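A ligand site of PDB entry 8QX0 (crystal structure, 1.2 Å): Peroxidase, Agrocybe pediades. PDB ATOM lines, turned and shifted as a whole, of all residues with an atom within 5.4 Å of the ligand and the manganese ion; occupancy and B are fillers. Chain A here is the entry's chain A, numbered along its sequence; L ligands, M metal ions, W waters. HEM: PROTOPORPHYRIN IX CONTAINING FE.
Three residues have an atom within 4 Å of the manganese ion: Asp 35, Asp 177 and Gln 333.
The nearest printed residue that does not touch the manganese ion is Gly 175 (5.1 Å).
O of Thr 78 lies close to O2A of the ligand, at 3.3 Å.
His 38 touches the ligand (O to CMD, 3.2 Å).
Leu 41 touches the ligand (O to CAC, 3.8 Å).
Phe 45 touches the ligand.
CB of Pro 140 touches CBB of the ligand (3.7 Å).
Glu 141 touches the ligand.
N of Pro 142 touches CMB of the ligand, 3.6 Å away.
Ile 149 touches the ligand.
Val 166 touches the ligand.
CD1 of Ile 167 touches CBB of the ligand, 3.7 Å away.
OG of Ser 170 touches CAC of the ligand (3.0 Å).
Val 173 touches the ligand (O to CMD, 3.9 Å).
Ala 174 touches the ligand (CB to CAD, 3.3 Å).
Ala 176 touches the ligand.
CG1 of Ile 179 touches O1A of the ligand, at 3.8 Å.
CE2 of Phe 188 touches CHA of the ligand (3.6 Å).
Leu 230 touches the ligand (CD1 to CHB, 3.7 Å).
Ser 232 touches the ligand (OG to CMB, 3.8 Å).
Ile 264 touches the ligand (CD1 to CBC, 3.8 Å).
Met 267 touches the ligand.
Hydrophobic or aromatic side chains within 4 Å of the ligand: His 38, Leu 41, Phe 45, Pro 140, Pro 142, Ile 149, Val 166, Ile 167, His 171, Ala 174, Ile 179, Phe 188, Leu 230, Ile 264 and Met 267.
Within 4 Å of the ligand: Asp 35, His 38, Leu 41, Arg 42, Phe 45, Thr 78, Pro 140, Glu 141, Pro 142, Ile 149, Val 166, Ile 167, Ser 170, His 171, Val 173, Ala 174, Gly 175, Ala 176, Asp 177, Asp 178, Ile 179, Phe 188, Leu 230, Ser 232, Ile 264 and Met 267.
N of Asp 177 sits at hydrogen-bond distance from O1A of the ligand (3.1 Å).
The side-chain carboxylate (OD2) of Asp 178 lies close to an oxygen (O2A) of the ligand, at 2.6 Å.
NH1 of Arg 42 is in salt-bridge range of O2A of the ligand (3.3 Å).
FE of the ligand is bound by NE2 of His 171, 2.1 Å away.
The backbone NH of Gly 175 is in hydrogen-bond range of an oxygen (O1D) of the ligand (3.0 Å).
N of Asp 178 sits at hydrogen-bond distance from O1A of the ligand (2.9 Å).
The guanidinium group (NH2) of Arg 42 sits at hydrogen-bond distance from the backbone carbonyl oxygen (O) of Thr 78, 2.9 Å away.
O of Val 173 sits at hydrogen-bond distance from ND1 of His 38 (3.0 Å).
The side-chain hydroxyl (OG) of Ser 170 sits at hydrogen-bond distance from the backbone carbonyl oxygen (O) of Val 166, at 2.9 Å.
The side-chain amide nitrogen (NE2) of Gln 333 lies within hydrogen-bond range of the backbone carbonyl oxygen (O) of Ile 331 (2.9 Å).
The backbone carbonyl oxygen of Pro 142 lies within hydrogen-bond range of the backbone NH of Ser 232, at 2.9 Å.
N of Phe 188 is in hydrogen-bond range of O of Ala 174, 3.2 Å away.
Water W5 lies within hydrogen-bond range of the side-chain carboxylate (OD1) of Asp 177 (2.7 Å), an oxygen (O1D) of the ligand (2.7 Å) and the side-chain amide nitrogen (NE2) of Gln 333 (2.9 Å).
Water W4 lies within hydrogen-bond range of the backbone carbonyl oxygen (O) of Gly 175 (2.7 Å), the backbone NH (N) of Asp 177 (3.0 Å) and an oxygen (O2A) of the ligand (3.2 Å).
The manganese ion is bound by the side-chain carboxylate (OD1) of Asp 35 (1.8 Å), the side-chain carboxylate (OD2) of Asp 177 (2.2 Å), an oxygen (O2D) of the ligand (2.2 Å), water W6 (2.2 Å), water W5 (2.3 Å) and the side-chain amide oxygen (OE1) of Gln 333 (2.3 Å).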
ATOM      1  N   ASP A  35     -12.830  -8.300 -40.045  1.00  0.00           N
ATOM      2  CA  ASP A  35     -11.928  -7.258 -39.557  1.00  0.00           C
ATOM      3  C   ASP A  35     -12.642  -5.909 -39.388  1.00  0.00           C
ATOM      4  O   ASP A  35     -12.255  -5.147 -38.518  1.00  0.00           O
ATOM      5  CB  ASP A  35     -10.698  -7.122 -40.443  1.00  0.00           C
ATOM      6  CG  ASP A  35      -9.650  -6.131 -39.912  1.00  0.00           C
ATOM      7  OD1 ASP A  35      -8.987  -6.182 -38.766  1.00  0.00           O
ATOM      8  OD2 ASP A  35      -9.322  -5.266 -40.746  1.00  0.00           O
ATOM      9  N   HIS A  38     -14.243  -6.153 -36.084  1.00  0.00           N
ATOM     10  CA  HIS A  38     -13.263  -6.104 -35.011  1.00  0.00           C
ATOM     11  C   HIS A  38     -12.773  -4.667 -34.827  1.00  0.00           C
ATOM     12  O   HIS A  38     -12.571  -4.189 -33.696  1.00  0.00           O
ATOM     13  CB  HIS A  38     -12.062  -6.993 -35.360  1.00  0.00           C
ATOM     14  CG  HIS A  38     -12.406  -8.423 -35.663  1.00  0.00           C
ATOM     15  ND1 HIS A  38     -13.569  -9.035 -35.278  1.00  0.00           N
ATOM     16  CD2 HIS A  38     -11.762  -9.328 -36.413  1.00  0.00           C
ATOM     17  CE1 HIS A  38     -13.585 -10.312 -35.689  1.00  0.00           C
ATOM     18  NE2 HIS A  38     -12.519 -10.504 -36.424  1.00  0.00           N
ATOM     19  N   GLY A  39     -12.528  -3.953 -35.921  1.00  0.00           N
ATOM     20  CA  GLY A  39     -12.037  -2.609 -35.817  1.00  0.00           C
ATOM     21  C   GLY A  39     -13.059  -1.690 -35.133  1.00  0.00           C
ATOM     22  O   GLY A  39     -12.705  -0.876 -34.316  1.00  0.00           O
ATOM     23  N   LEU A  41     -15.336  -2.556 -32.995  1.00  0.00           N
ATOM     24  CA  LEU A  41     -15.348  -2.876 -31.571  1.00  0.00           C
ATOM     25  C   LEU A  41     -14.125  -2.296 -30.867  1.00  0.00           C
ATOM     26  O   LEU A  41     -14.272  -1.743 -29.777  1.00  0.00           O
ATOM     27  CB  LEU A  41     -15.453  -4.399 -31.392  1.00  0.00           C
ATOM     28  CG  LEU A  41     -15.481  -4.887 -29.945  1.00  0.00           C
ATOM     29  CD1 LEU A  41     -16.669  -4.316 -29.149  1.00  0.00           C
ATOM     30  CD2 LEU A  41     -15.505  -6.399 -29.891  1.00  0.00           C
ATOM     31  N   ARG A  42     -12.904  -2.461 -31.402  1.00  0.00           N
ATOM     32  CA  ARG A  42     -11.710  -1.891 -30.801  1.00  0.00           C
ATOM     33  C   ARG A  42     -11.902  -0.392 -30.614  1.00  0.00           C
ATOM     34  O   ARG A  42     -11.416   0.178 -29.637  1.00  0.00           O
ATOM     35  CB  ARG A  42     -10.488  -2.288 -31.632  1.00  0.00           C
ATOM     36  CG  ARG A  42      -9.196  -1.875 -30.969  1.00  0.00           C
ATOM     37  CD  ARG A  42      -7.950  -2.326 -31.790  1.00  0.00           C
ATOM     38  NE  ARG A  42      -6.739  -1.789 -31.168  1.00  0.00           N
ATOM     39  CZ  ARG A  42      -5.673  -1.349 -31.775  1.00  0.00           C
ATOM     40  NH1 ARG A  42      -5.630  -1.329 -33.098  1.00  0.00           N
ATOM     41  NH2 ARG A  42      -4.665  -0.872 -31.064  1.00  0.00           N
ATOM     42  N   VAL A  44     -14.435   1.413 -29.998  1.00  0.00           N
ATOM     43  CA  VAL A  44     -15.182   1.742 -28.793  1.00  0.00           C
ATOM     44  C   VAL A  44     -14.244   1.948 -27.613  1.00  0.00           C
ATOM     45  O   VAL A  44     -14.358   2.946 -26.868  1.00  0.00           O
ATOM     46  CB  VAL A  44     -16.181   0.620 -28.502  1.00  0.00           C
ATOM     47  CG1 VAL A  44     -16.768   0.660 -27.085  1.00  0.00           C
ATOM     48  CG2 VAL A  44     -17.315   0.598 -29.493  1.00  0.00           C
ATOM     49  N   PHE A  45     -13.341   0.971 -27.410  1.00  0.00           N
ATOM     50  CA  PHE A  45     -12.394   1.044 -26.308  1.00  0.00           C
ATOM     51  C   PHE A  45     -11.473   2.245 -26.416  1.00  0.00           C
ATOM     52  O   PHE A  45     -11.276   2.985 -25.468  1.00  0.00           O
ATOM     53  CB  PHE A  45     -11.635  -0.284 -26.290  1.00  0.00           C
ATOM     54  CG  PHE A  45     -10.599  -0.429 -25.197  1.00  0.00           C
ATOM     55  CD1 PHE A  45     -10.935  -0.188 -23.875  1.00  0.00           C
ATOM     56  CD2 PHE A  45      -9.297  -0.749 -25.514  1.00  0.00           C
ATOM     57  CE1 PHE A  45      -9.968  -0.352 -22.901  1.00  0.00           C
ATOM     58  CE2 PHE A  45      -8.323  -0.870 -24.507  1.00  0.00           C
ATOM     59  CZ  PHE A  45      -8.707  -0.668 -23.220  1.00  0.00           C
ATOM     60  N   THR A  78      -1.666   2.420 -31.764  1.00  0.00           N
ATOM     61  CA  THR A  78      -1.106   1.814 -32.960  1.00  0.00           C
ATOM     62  C   THR A  78      -2.192   0.994 -33.668  1.00  0.00           C
ATOM     63  O   THR A  78      -2.896   0.187 -33.074  1.00  0.00           O
ATOM     64  CB  THR A  78       0.108   0.948 -32.581  1.00  0.00           C
ATOM     65  OG1 THR A  78       1.122   1.764 -32.016  1.00  0.00           O
ATOM     66  CG2 THR A  78       0.688   0.220 -33.764  1.00  0.00           C
ATOM     67  N   GLY A  79      -2.308   1.146 -34.987  1.00  0.00           N
ATOM     68  CA  GLY A  79      -3.256   0.374 -35.757  1.00  0.00           C
ATOM     69  C   GLY A  79      -4.663   0.990 -35.853  1.00  0.00           C
ATOM     70  O   GLY A  79      -5.477   0.586 -36.670  1.00  0.00           O
ATOM     71  N   VAL A  83      -7.963   1.078 -38.713  1.00  0.00           N
ATOM     72  CA  VAL A  83      -9.376   0.992 -38.372  1.00  0.00           C
ATOM     73  C   VAL A  83     -10.130   2.210 -38.923  1.00  0.00           C
ATOM     74  O   VAL A  83     -11.202   2.080 -39.514  1.00  0.00           O
ATOM     75  CB  VAL A  83      -9.565   0.890 -36.853  1.00  0.00           C
ATOM     76  CG1 VAL A  83     -11.050   0.963 -36.498  1.00  0.00           C
ATOM     77  CG2 VAL A  83      -8.971  -0.397 -36.305  1.00  0.00           C
ATOM     78  N   PRO A 140      -4.829   1.614 -21.856  1.00  0.00           N
ATOM     79  CA  PRO A 140      -3.946   0.541 -21.412  1.00  0.00           C
ATOM     80  C   PRO A 140      -3.187  -0.131 -22.532  1.00  0.00           C
ATOM     81  O   PRO A 140      -3.686  -0.323 -23.641  1.00  0.00           O
ATOM     82  CB  PRO A 140      -4.933  -0.440 -20.753  1.00  0.00           C
ATOM     83  CG  PRO A 140      -6.033   0.437 -20.231  1.00  0.00           C
ATOM     84  CD  PRO A 140      -6.210   1.452 -21.346  1.00  0.00           C
ATOM     85  N   GLU A 141      -1.954  -0.522 -22.195  1.00  0.00           N
ATOM     86  CA  GLU A 141      -1.048  -1.233 -23.092  1.00  0.00           C
ATOM     87  C   GLU A 141      -0.958  -2.673 -22.682  1.00  0.00           C
ATOM     88  O   GLU A 141      -1.150  -3.045 -21.535  1.00  0.00           O
ATOM     89  CB  GLU A 141       0.338  -0.614 -22.899  1.00  0.00           C
ATOM     90  CG  GLU A 141       0.530   0.794 -23.475  1.00  0.00           C
ATOM     91  CD  GLU A 141       0.910   0.853 -24.946  1.00  0.00           C
ATOM     92  OE1 GLU A 141       0.763  -0.164 -25.610  1.00  0.00           O
ATOM     93  OE2 GLU A 141       1.386   1.935 -25.378  1.00  0.00           O
ATOM     94  N   PRO A 142      -0.566  -3.567 -23.618  1.00  0.00           N
ATOM     95  CA  PRO A 142      -0.478  -4.991 -23.352  1.00  0.00           C
ATOM     96  C   PRO A 142       0.663  -5.360 -22.402  1.00  0.00           C
ATOM     97  O   PRO A 142       0.648  -6.461 -21.827  1.00  0.00           O
ATOM     98  CB  PRO A 142      -0.291  -5.630 -24.699  1.00  0.00           C
ATOM     99  CG  PRO A 142       0.294  -4.540 -25.562  1.00  0.00           C
ATOM    100  CD  PRO A 142      -0.366  -3.279 -25.054  1.00  0.00           C
ATOM    101  N   ILE A 149      -3.941  -2.041 -14.792  1.00  0.00           N
ATOM    102  CA  ILE A 149      -5.162  -2.231 -15.544  1.00  0.00           C
ATOM    103  C   ILE A 149      -6.325  -2.065 -14.611  1.00  0.00           C
ATOM    104  O   ILE A 149      -7.309  -1.414 -14.955  1.00  0.00           O
ATOM    105  CB  ILE A 149      -5.159  -3.598 -16.237  1.00  0.00           C
ATOM    106  CG1 ILE A 149      -4.092  -3.607 -17.350  1.00  0.00           C
ATOM    107  CG2 ILE A 149      -6.535  -3.988 -16.761  1.00  0.00           C
ATOM    108  CD1 ILE A 149      -3.808  -4.966 -17.932  1.00  0.00           C
ATOM    109  N   PHE A 153      -9.420   0.726 -14.980  1.00  0.00           N
ATOM    110  CA  PHE A 153     -10.814   0.361 -15.095  1.00  0.00           C
ATOM    111  C   PHE A 153     -11.558   0.652 -13.807  1.00  0.00           C
ATOM    112  O   PHE A 153     -12.701   1.138 -13.850  1.00  0.00           O
ATOM    113  CB  PHE A 153     -10.989  -1.087 -15.469  1.00  0.00           C
ATOM    114  CG  PHE A 153     -10.757  -1.402 -16.949  1.00  0.00           C
ATOM    115  CD1 PHE A 153      -9.491  -1.519 -17.511  1.00  0.00           C
ATOM    116  CD2 PHE A 153     -11.838  -1.656 -17.772  1.00  0.00           C
ATOM    117  CE1 PHE A 153      -9.354  -1.837 -18.850  1.00  0.00           C
ATOM    118  CE2 PHE A 153     -11.679  -1.900 -19.126  1.00  0.00           C
ATOM    119  CZ  PHE A 153     -10.454  -2.081 -19.636  1.00  0.00           C
ATOM    120  N   VAL A 166     -14.990  -7.731 -20.339  1.00  0.00           N
ATOM    121  CA  VAL A 166     -14.962  -6.835 -21.498  1.00  0.00           C
ATOM    122  C   VAL A 166     -13.647  -7.048 -22.264  1.00  0.00           C
ATOM    123  O   VAL A 166     -13.630  -6.951 -23.477  1.00  0.00           O
ATOM    124  CB  VAL A 166     -15.293  -5.368 -21.165  1.00  0.00           C
ATOM    125  CG1 VAL A 166     -14.159  -4.656 -20.495  1.00  0.00           C
ATOM    126  CG2 VAL A 166     -15.856  -4.602 -22.373  1.00  0.00           C
ATOM    127  N   ILE A 167     -12.551  -7.251 -21.556  1.00  0.00           N
ATOM    128  CA  ILE A 167     -11.243  -7.516 -22.175  1.00  0.00           C
ATOM    129  C   ILE A 167     -11.279  -8.882 -22.834  1.00  0.00           C
ATOM    130  O   ILE A 167     -11.043  -8.989 -24.042  1.00  0.00           O
ATOM    131  CB  ILE A 167     -10.088  -7.332 -21.191  1.00  0.00           C
ATOM    132  CG1 ILE A 167     -10.057  -5.966 -20.583  1.00  0.00           C
ATOM    133  CG2 ILE A 167      -8.742  -7.668 -21.864  1.00  0.00           C
ATOM    134  CD1 ILE A 167      -9.112  -5.804 -19.415  1.00  0.00           C
ATOM    135  N   SER A 170     -13.921  -9.334 -25.661  1.00  0.00           N
ATOM    136  CA  SER A 170     -13.536  -8.662 -26.882  1.00  0.00           C
ATOM    137  C   SER A 170     -12.509  -9.506 -27.652  1.00  0.00           C
ATOM    138  O   SER A 170     -12.509  -9.543 -28.888  1.00  0.00           O
ATOM    139  CB  SER A 170     -13.059  -7.291 -26.665  1.00  0.00           C
ATOM    140  OG  SER A 170     -14.132  -6.442 -26.236  1.00  0.00           O
ATOM    141  N   HIS A 171     -11.540 -10.058 -26.926  1.00  0.00           N
ATOM    142  CA  HIS A 171     -10.447 -10.795 -27.512  1.00  0.00           C
ATOM    143  C   HIS A 171     -10.878 -12.140 -28.044  1.00  0.00           C
ATOM    144  O   HIS A 171     -10.107 -12.754 -28.768  1.00  0.00           O
ATOM    145  CB  HIS A 171      -9.223 -10.771 -26.593  1.00  0.00           C
ATOM    146  CG  HIS A 171      -8.565  -9.429 -26.476  1.00  0.00           C
ATOM    147  ND1 HIS A 171      -7.497  -9.158 -25.649  1.00  0.00           N
ATOM    148  CD2 HIS A 171      -8.876  -8.178 -27.035  1.00  0.00           C
ATOM    149  CE1 HIS A 171      -7.235  -7.856 -25.722  1.00  0.00           C
ATOM    150  NE2 HIS A 171      -8.012  -7.256 -26.570  1.00  0.00           N
ATOM    151  N   VAL A 173     -13.065 -12.141 -30.330  1.00  0.00           N
ATOM    152  CA  VAL A 173     -13.453 -11.779 -31.676  1.00  0.00           C
ATOM    153  C   VAL A 173     -12.475 -10.694 -32.175  1.00  0.00           C
ATOM    154  O   VAL A 173     -12.826  -9.512 -32.371  1.00  0.00           O
ATOM    155  CB  VAL A 173     -14.928 -11.328 -31.735  1.00  0.00           C
ATOM    156  CG1 VAL A 173     -15.867 -12.528 -31.639  1.00  0.00           C
ATOM    157  CG2 VAL A 173     -15.273 -10.275 -30.705  1.00  0.00           C
ATOM    158  N   ALA A 174     -11.199 -11.098 -32.349  1.00  0.00           N
ATOM    159  CA  ALA A 174     -10.138 -10.101 -32.455  1.00  0.00           C
ATOM    160  C   ALA A 174      -8.843 -10.716 -32.911  1.00  0.00           C
ATOM    161  O   ALA A 174      -8.517 -11.866 -32.609  1.00  0.00           O
ATOM    162  CB  ALA A 174      -9.871  -9.455 -31.111  1.00  0.00           C
ATOM    163  N   GLY A 175      -8.067  -9.874 -33.599  1.00  0.00           N
ATOM    164  CA  GLY A 175      -6.700 -10.253 -33.903  1.00  0.00           C
ATOM    165  C   GLY A 175      -5.715  -9.110 -33.711  1.00  0.00           C
ATOM    166  O   GLY A 175      -6.098  -7.933 -33.569  1.00  0.00           O
ATOM    167  N   ALA A 176      -4.429  -9.443 -33.764  1.00  0.00           N
ATOM    168  CA  ALA A 176      -3.334  -8.500 -33.589  1.00  0.00           C
ATOM    169  C   ALA A 176      -2.698  -8.218 -34.933  1.00  0.00           C
ATOM    170  O   ALA A 176      -2.288  -9.170 -35.636  1.00  0.00           O
ATOM    171  CB  ALA A 176      -2.299  -9.043 -32.676  1.00  0.00           C
ATOM    172  N   ASP A 177      -2.621  -6.947 -35.273  1.00  0.00           N
ATOM    173  CA  ASP A 177      -2.130  -6.474 -36.563  1.00  0.00           C
ATOM    174  C   ASP A 177      -0.746  -5.878 -36.482  1.00  0.00           C
ATOM    175  O   ASP A 177      -0.100  -5.749 -37.546  1.00  0.00           O
ATOM    176  CB  ASP A 177      -3.136  -5.485 -37.107  1.00  0.00           C
ATOM    177  CG  ASP A 177      -4.509  -6.075 -37.360  1.00  0.00           C
ATOM    178  OD1 ASP A 177      -4.629  -7.355 -37.431  1.00  0.00           O
ATOM    179  OD2 ASP A 177      -5.451  -5.237 -37.396  1.00  0.00           O
ATOM    180  N   ASP A 178      -0.269  -5.507 -35.313  1.00  0.00           N
ATOM    181  CA  ASP A 178       0.926  -4.710 -35.086  1.00  0.00           C
ATOM    182  C   ASP A 178       1.785  -5.351 -33.997  1.00  0.00           C
ATOM    183  O   ASP A 178       2.657  -4.648 -33.426  1.00  0.00           O
ATOM    184  CB  ASP A 178       0.580  -3.274 -34.765  1.00  0.00           C
ATOM    185  CG  ASP A 178      -0.299  -2.626 -35.831  1.00  0.00           C
ATOM    186  OD1 ASP A 178       0.301  -2.191 -36.862  1.00  0.00           O
ATOM    187  OD2 ASP A 178      -1.540  -2.655 -35.744  1.00  0.00           O
ATOM    188  N   ILE A 179       1.599  -6.626 -33.728  1.00  0.00           N
ATOM    189  CA  ILE A 179       2.369  -7.355 -32.729  1.00  0.00           C
ATOM    190  C   ILE A 179       3.348  -8.346 -33.352  1.00  0.00           C
ATOM    191  O   ILE A 179       4.528  -8.327 -33.000  1.00  0.00           O
ATOM    192  CB  ILE A 179       1.425  -8.057 -31.742  1.00  0.00           C
ATOM    193  CG1 ILE A 179       0.500  -7.084 -30.990  1.00  0.00           C
ATOM    194  CG2 ILE A 179       2.203  -8.956 -30.789  1.00  0.00           C
ATOM    195  CD1 ILE A 179       1.220  -6.134 -30.054  1.00  0.00           C
ATOM    196  N   PHE A 188      -6.350 -13.822 -31.394  1.00  0.00           N
ATOM    197  CA  PHE A 188      -6.079 -14.139 -30.013  1.00  0.00           C
ATOM    198  C   PHE A 188      -6.679 -15.483 -29.577  1.00  0.00           C
ATOM    199  O   PHE A 188      -6.131 -16.151 -28.693  1.00  0.00           O
ATOM    200  CB  PHE A 188      -6.607 -13.078 -29.054  1.00  0.00           C
ATOM    201  CG  PHE A 188      -5.992 -11.707 -29.322  1.00  0.00           C
ATOM    202  CD1 PHE A 188      -4.619 -11.483 -29.197  1.00  0.00           C
ATOM    203  CD2 PHE A 188      -6.805 -10.596 -29.550  1.00  0.00           C
ATOM    204  CE1 PHE A 188      -4.054 -10.227 -29.436  1.00  0.00           C
ATOM    205  CE2 PHE A 188      -6.256  -9.349 -29.740  1.00  0.00           C
ATOM    206  CZ  PHE A 188      -4.878  -9.149 -29.698  1.00  0.00           C
ATOM    207  N   LEU A 230      -1.291 -11.814 -25.647  1.00  0.00           N
ATOM    208  CA  LEU A 230      -0.855 -10.586 -24.990  1.00  0.00           C
ATOM    209  C   LEU A 230      -0.427 -10.930 -23.581  1.00  0.00           C
ATOM    210  O   LEU A 230      -1.087 -11.680 -22.845  1.00  0.00           O
ATOM    211  CB  LEU A 230      -2.011  -9.598 -24.974  1.00  0.00           C
ATOM    212  CG  LEU A 230      -2.546  -9.192 -26.339  1.00  0.00           C
ATOM    213  CD1 LEU A 230      -3.688  -8.231 -26.149  1.00  0.00           C
ATOM    214  CD2 LEU A 230      -1.514  -8.647 -27.307  1.00  0.00           C
ATOM    215  N   SER A 232      -0.851  -8.870 -21.078  1.00  0.00           N
ATOM    216  CA  SER A 232      -1.957  -8.435 -20.252  1.00  0.00           C
ATOM    217  C   SER A 232      -2.964  -9.549 -20.013  1.00  0.00           C
ATOM    218  O   SER A 232      -3.412  -9.814 -18.893  1.00  0.00           O
ATOM    219  CB  SER A 232      -2.606  -7.167 -20.838  1.00  0.00           C
ATOM    220  OG  SER A 232      -2.839  -7.375 -22.217  1.00  0.00           O
ATOM    221  N   LEU A 236      -3.823 -11.449 -16.577  1.00  0.00           N
ATOM    222  CA  LEU A 236      -5.185 -11.415 -16.061  1.00  0.00           C
ATOM    223  C   LEU A 236      -5.668 -12.836 -15.712  1.00  0.00           C
ATOM    224  O   LEU A 236      -6.361 -13.032 -14.720  1.00  0.00           O
ATOM    225  CB  LEU A 236      -6.171 -10.734 -17.002  1.00  0.00           C
ATOM    226  CG  LEU A 236      -6.030  -9.213 -17.098  1.00  0.00           C
ATOM    227  CD1 LEU A 236      -6.700  -8.630 -18.333  1.00  0.00           C
ATOM    228  CD2 LEU A 236      -6.595  -8.560 -15.817  1.00  0.00           C
ATOM    229  N   ILE A 264     -20.004  -3.111 -21.868  1.00  0.00           N
ATOM    230  CA  ILE A 264     -19.935  -2.257 -23.052  1.00  0.00           C
ATOM    231  C   ILE A 264     -20.847  -1.042 -22.856  1.00  0.00           C
ATOM    232  O   ILE A 264     -20.486   0.075 -23.192  1.00  0.00           O
ATOM    233  CB  ILE A 264     -20.316  -3.056 -24.304  1.00  0.00           C
ATOM    234  CG1 ILE A 264     -19.240  -4.079 -24.675  1.00  0.00           C
ATOM    235  CG2 ILE A 264     -20.623  -2.147 -25.513  1.00  0.00           C
ATOM    236  CD1 ILE A 264     -17.928  -3.511 -25.218  1.00  0.00           C
ATOM    237  N   MET A 267     -19.200   1.333 -20.627  1.00  0.00           N
ATOM    238  CA  MET A 267     -18.111   1.996 -21.331  1.00  0.00           C
ATOM    239  C   MET A 267     -18.641   3.108 -22.249  1.00  0.00           C
ATOM    240  O   MET A 267     -17.997   4.141 -22.384  1.00  0.00           O
ATOM    241  CB  MET A 267     -17.379   0.902 -22.112  1.00  0.00           C
ATOM    242  CG  MET A 267     -16.110   1.340 -22.778  1.00  0.00           C
ATOM    243  SD  MET A 267     -15.058   0.059 -23.464  1.00  0.00           S
ATOM    244  CE  MET A 267     -14.562  -0.790 -21.959  1.00  0.00           C
ATOM    245  N   ILE A 331      -6.845 -13.448 -40.168  1.00  0.00           N
ATOM    246  CA  ILE A 331      -8.033 -12.668 -40.478  1.00  0.00           C
ATOM    247  C   ILE A 331      -7.701 -11.729 -41.627  1.00  0.00           C
ATOM    248  O   ILE A 331      -6.811 -10.896 -41.512  1.00  0.00           O
ATOM    249  CB  ILE A 331      -8.465 -11.793 -39.258  1.00  0.00           C
ATOM    250  CG1 ILE A 331      -8.730 -12.657 -38.035  1.00  0.00           C
ATOM    251  CG2 ILE A 331      -9.679 -10.956 -39.616  1.00  0.00           C
ATOM    252  CD1 ILE A 331      -8.662 -11.884 -36.738  1.00  0.00           C
ATOM    253  N   GLN A 333      -7.706  -8.491 -43.749  1.00  0.00           N
ATOM    254  CA  GLN A 333      -7.890  -7.138 -43.246  1.00  0.00           C
ATOM    255  C   GLN A 333      -8.823  -6.352 -44.155  1.00  0.00           C
ATOM    256  O   GLN A 333      -8.736  -6.472 -45.390  1.00  0.00           O
ATOM    257  CB  GLN A 333      -6.505  -6.552 -43.046  1.00  0.00           C
ATOM    258  CG  GLN A 333      -5.692  -7.233 -41.954  1.00  0.00           C
ATOM    259  CD  GLN A 333      -6.409  -7.194 -40.599  1.00  0.00           C
ATOM    260  OE1 GLN A 333      -6.467  -6.134 -39.945  1.00  0.00           O
ATOM    261  NE2 GLN A 333      -6.915  -8.325 -40.179  1.00  0.00           N
HETATM  262  CHA HEM L   1      -6.853  -5.819 -30.331  1.00  0.00           C
HETATM  263  CHB HEM L   1      -4.739  -4.721 -26.116  1.00  0.00           C
HETATM  264  CHC HEM L   1      -9.074  -4.177 -24.069  1.00  0.00           C
HETATM  265  CHD HEM L   1     -11.132  -4.827 -28.375  1.00  0.00           C
HETATM  266  C1A HEM L   1      -5.882  -5.500 -29.383  1.00  0.00           C
HETATM  267  C2A HEM L   1      -4.470  -5.465 -29.585  1.00  0.00           C
HETATM  268  C3A HEM L   1      -3.861  -5.152 -28.442  1.00  0.00           C
HETATM  269  C4A HEM L   1      -4.912  -4.985 -27.461  1.00  0.00           C
HETATM  270  CMA HEM L   1      -2.369  -4.913 -28.155  1.00  0.00           C
HETATM  271  CAA HEM L   1      -3.750  -5.574 -30.909  1.00  0.00           C
HETATM  272  CBA HEM L   1      -3.636  -4.154 -31.594  1.00  0.00           C
HETATM  273  CGA HEM L   1      -2.762  -4.102 -32.767  1.00  0.00           C
HETATM  274  O1A HEM L   1      -1.901  -5.005 -33.004  1.00  0.00           O
HETATM  275  O2A HEM L   1      -2.935  -3.096 -33.593  1.00  0.00           O
HETATM  276  C1B HEM L   1      -5.713  -4.508 -25.128  1.00  0.00           C
HETATM  277  C2B HEM L   1      -5.429  -4.192 -23.754  1.00  0.00           C
HETATM  278  C3B HEM L   1      -6.674  -4.072 -23.166  1.00  0.00           C
HETATM  279  C4B HEM L   1      -7.669  -4.356 -24.223  1.00  0.00           C
HETATM  280  CMB HEM L   1      -4.114  -3.964 -23.128  1.00  0.00           C
HETATM  281  CAB HEM L   1      -7.053  -3.761 -21.782  1.00  0.00           C
HETATM  282  CBB HEM L   1      -6.270  -3.876 -20.660  1.00  0.00           C
HETATM  283  C1C HEM L   1     -10.067  -4.260 -25.058  1.00  0.00           C
HETATM  284  C2C HEM L   1     -11.427  -3.844 -24.926  1.00  0.00           C
HETATM  285  C3C HEM L   1     -12.028  -3.954 -26.129  1.00  0.00           C
HETATM  286  C4C HEM L   1     -10.987  -4.471 -27.065  1.00  0.00           C
HETATM  287  CMC HEM L   1     -12.089  -3.485 -23.638  1.00  0.00           C
HETATM  288  CAC HEM L   1     -13.387  -3.605 -26.577  1.00  0.00           C
HETATM  289  CBC HEM L   1     -14.270  -2.917 -25.906  1.00  0.00           C
HETATM  290  C1D HEM L   1     -10.165  -5.296 -29.246  1.00  0.00           C
HETATM  291  C2D HEM L   1     -10.494  -5.759 -30.591  1.00  0.00           C
HETATM  292  C3D HEM L   1      -9.266  -6.025 -31.095  1.00  0.00           C
HETATM  293  C4D HEM L   1      -8.245  -5.657 -30.123  1.00  0.00           C
HETATM  294  CMD HEM L   1     -11.792  -5.982 -31.169  1.00  0.00           C
HETATM  295  CAD HEM L   1      -8.990  -6.550 -32.506  1.00  0.00           C
HETATM  296  CBD HEM L   1      -8.796  -5.553 -33.619  1.00  0.00           C
HETATM  297  CGD HEM L   1      -8.555  -6.179 -35.014  1.00  0.00           C
HETATM  298  O1D HEM L   1      -8.768  -7.371 -35.175  1.00  0.00           O
HETATM  299  O2D HEM L   1      -8.178  -5.390 -35.895  1.00  0.00           O
HETATM  300  NA  HEM L   1      -6.118  -5.224 -28.040  1.00  0.00           N
HETATM  301  NB  HEM L   1      -7.014  -4.595 -25.445  1.00  0.00           N
HETATM  302  NC  HEM L   1      -9.761  -4.539 -26.403  1.00  0.00           N
HETATM  303  ND  HEM L   1      -8.845  -5.242 -28.968  1.00  0.00           N
HETATM  304 FE   HEM L   1      -7.981  -5.206 -27.122  1.00  0.00          FE
HETATM  305 MN    MN M   1      -7.504  -5.702 -37.949  1.00  0.00          MN
HETATM  306  O   HOH W   1      -6.626  -3.261 -34.983  1.00  0.00           O
HETATM  307  O   HOH W   2      -3.432  -1.587 -26.040  1.00  0.00           O
HETATM  308  O   HOH W   3      -4.921  -1.925 -28.189  1.00  0.00           O
HETATM  309  O   HOH W   4      -4.967  -5.520 -34.162  1.00  0.00           O
HETATM  310  O   HOH W   5      -7.258  -7.893 -37.372  1.00  0.00           O
HETATM  311  O   HOH W   6      -7.687  -3.549 -38.356  1.00  0.00           O
HETATM  312  O   HOH W   7      -5.445  -7.307 -22.676  1.00  0.00           O
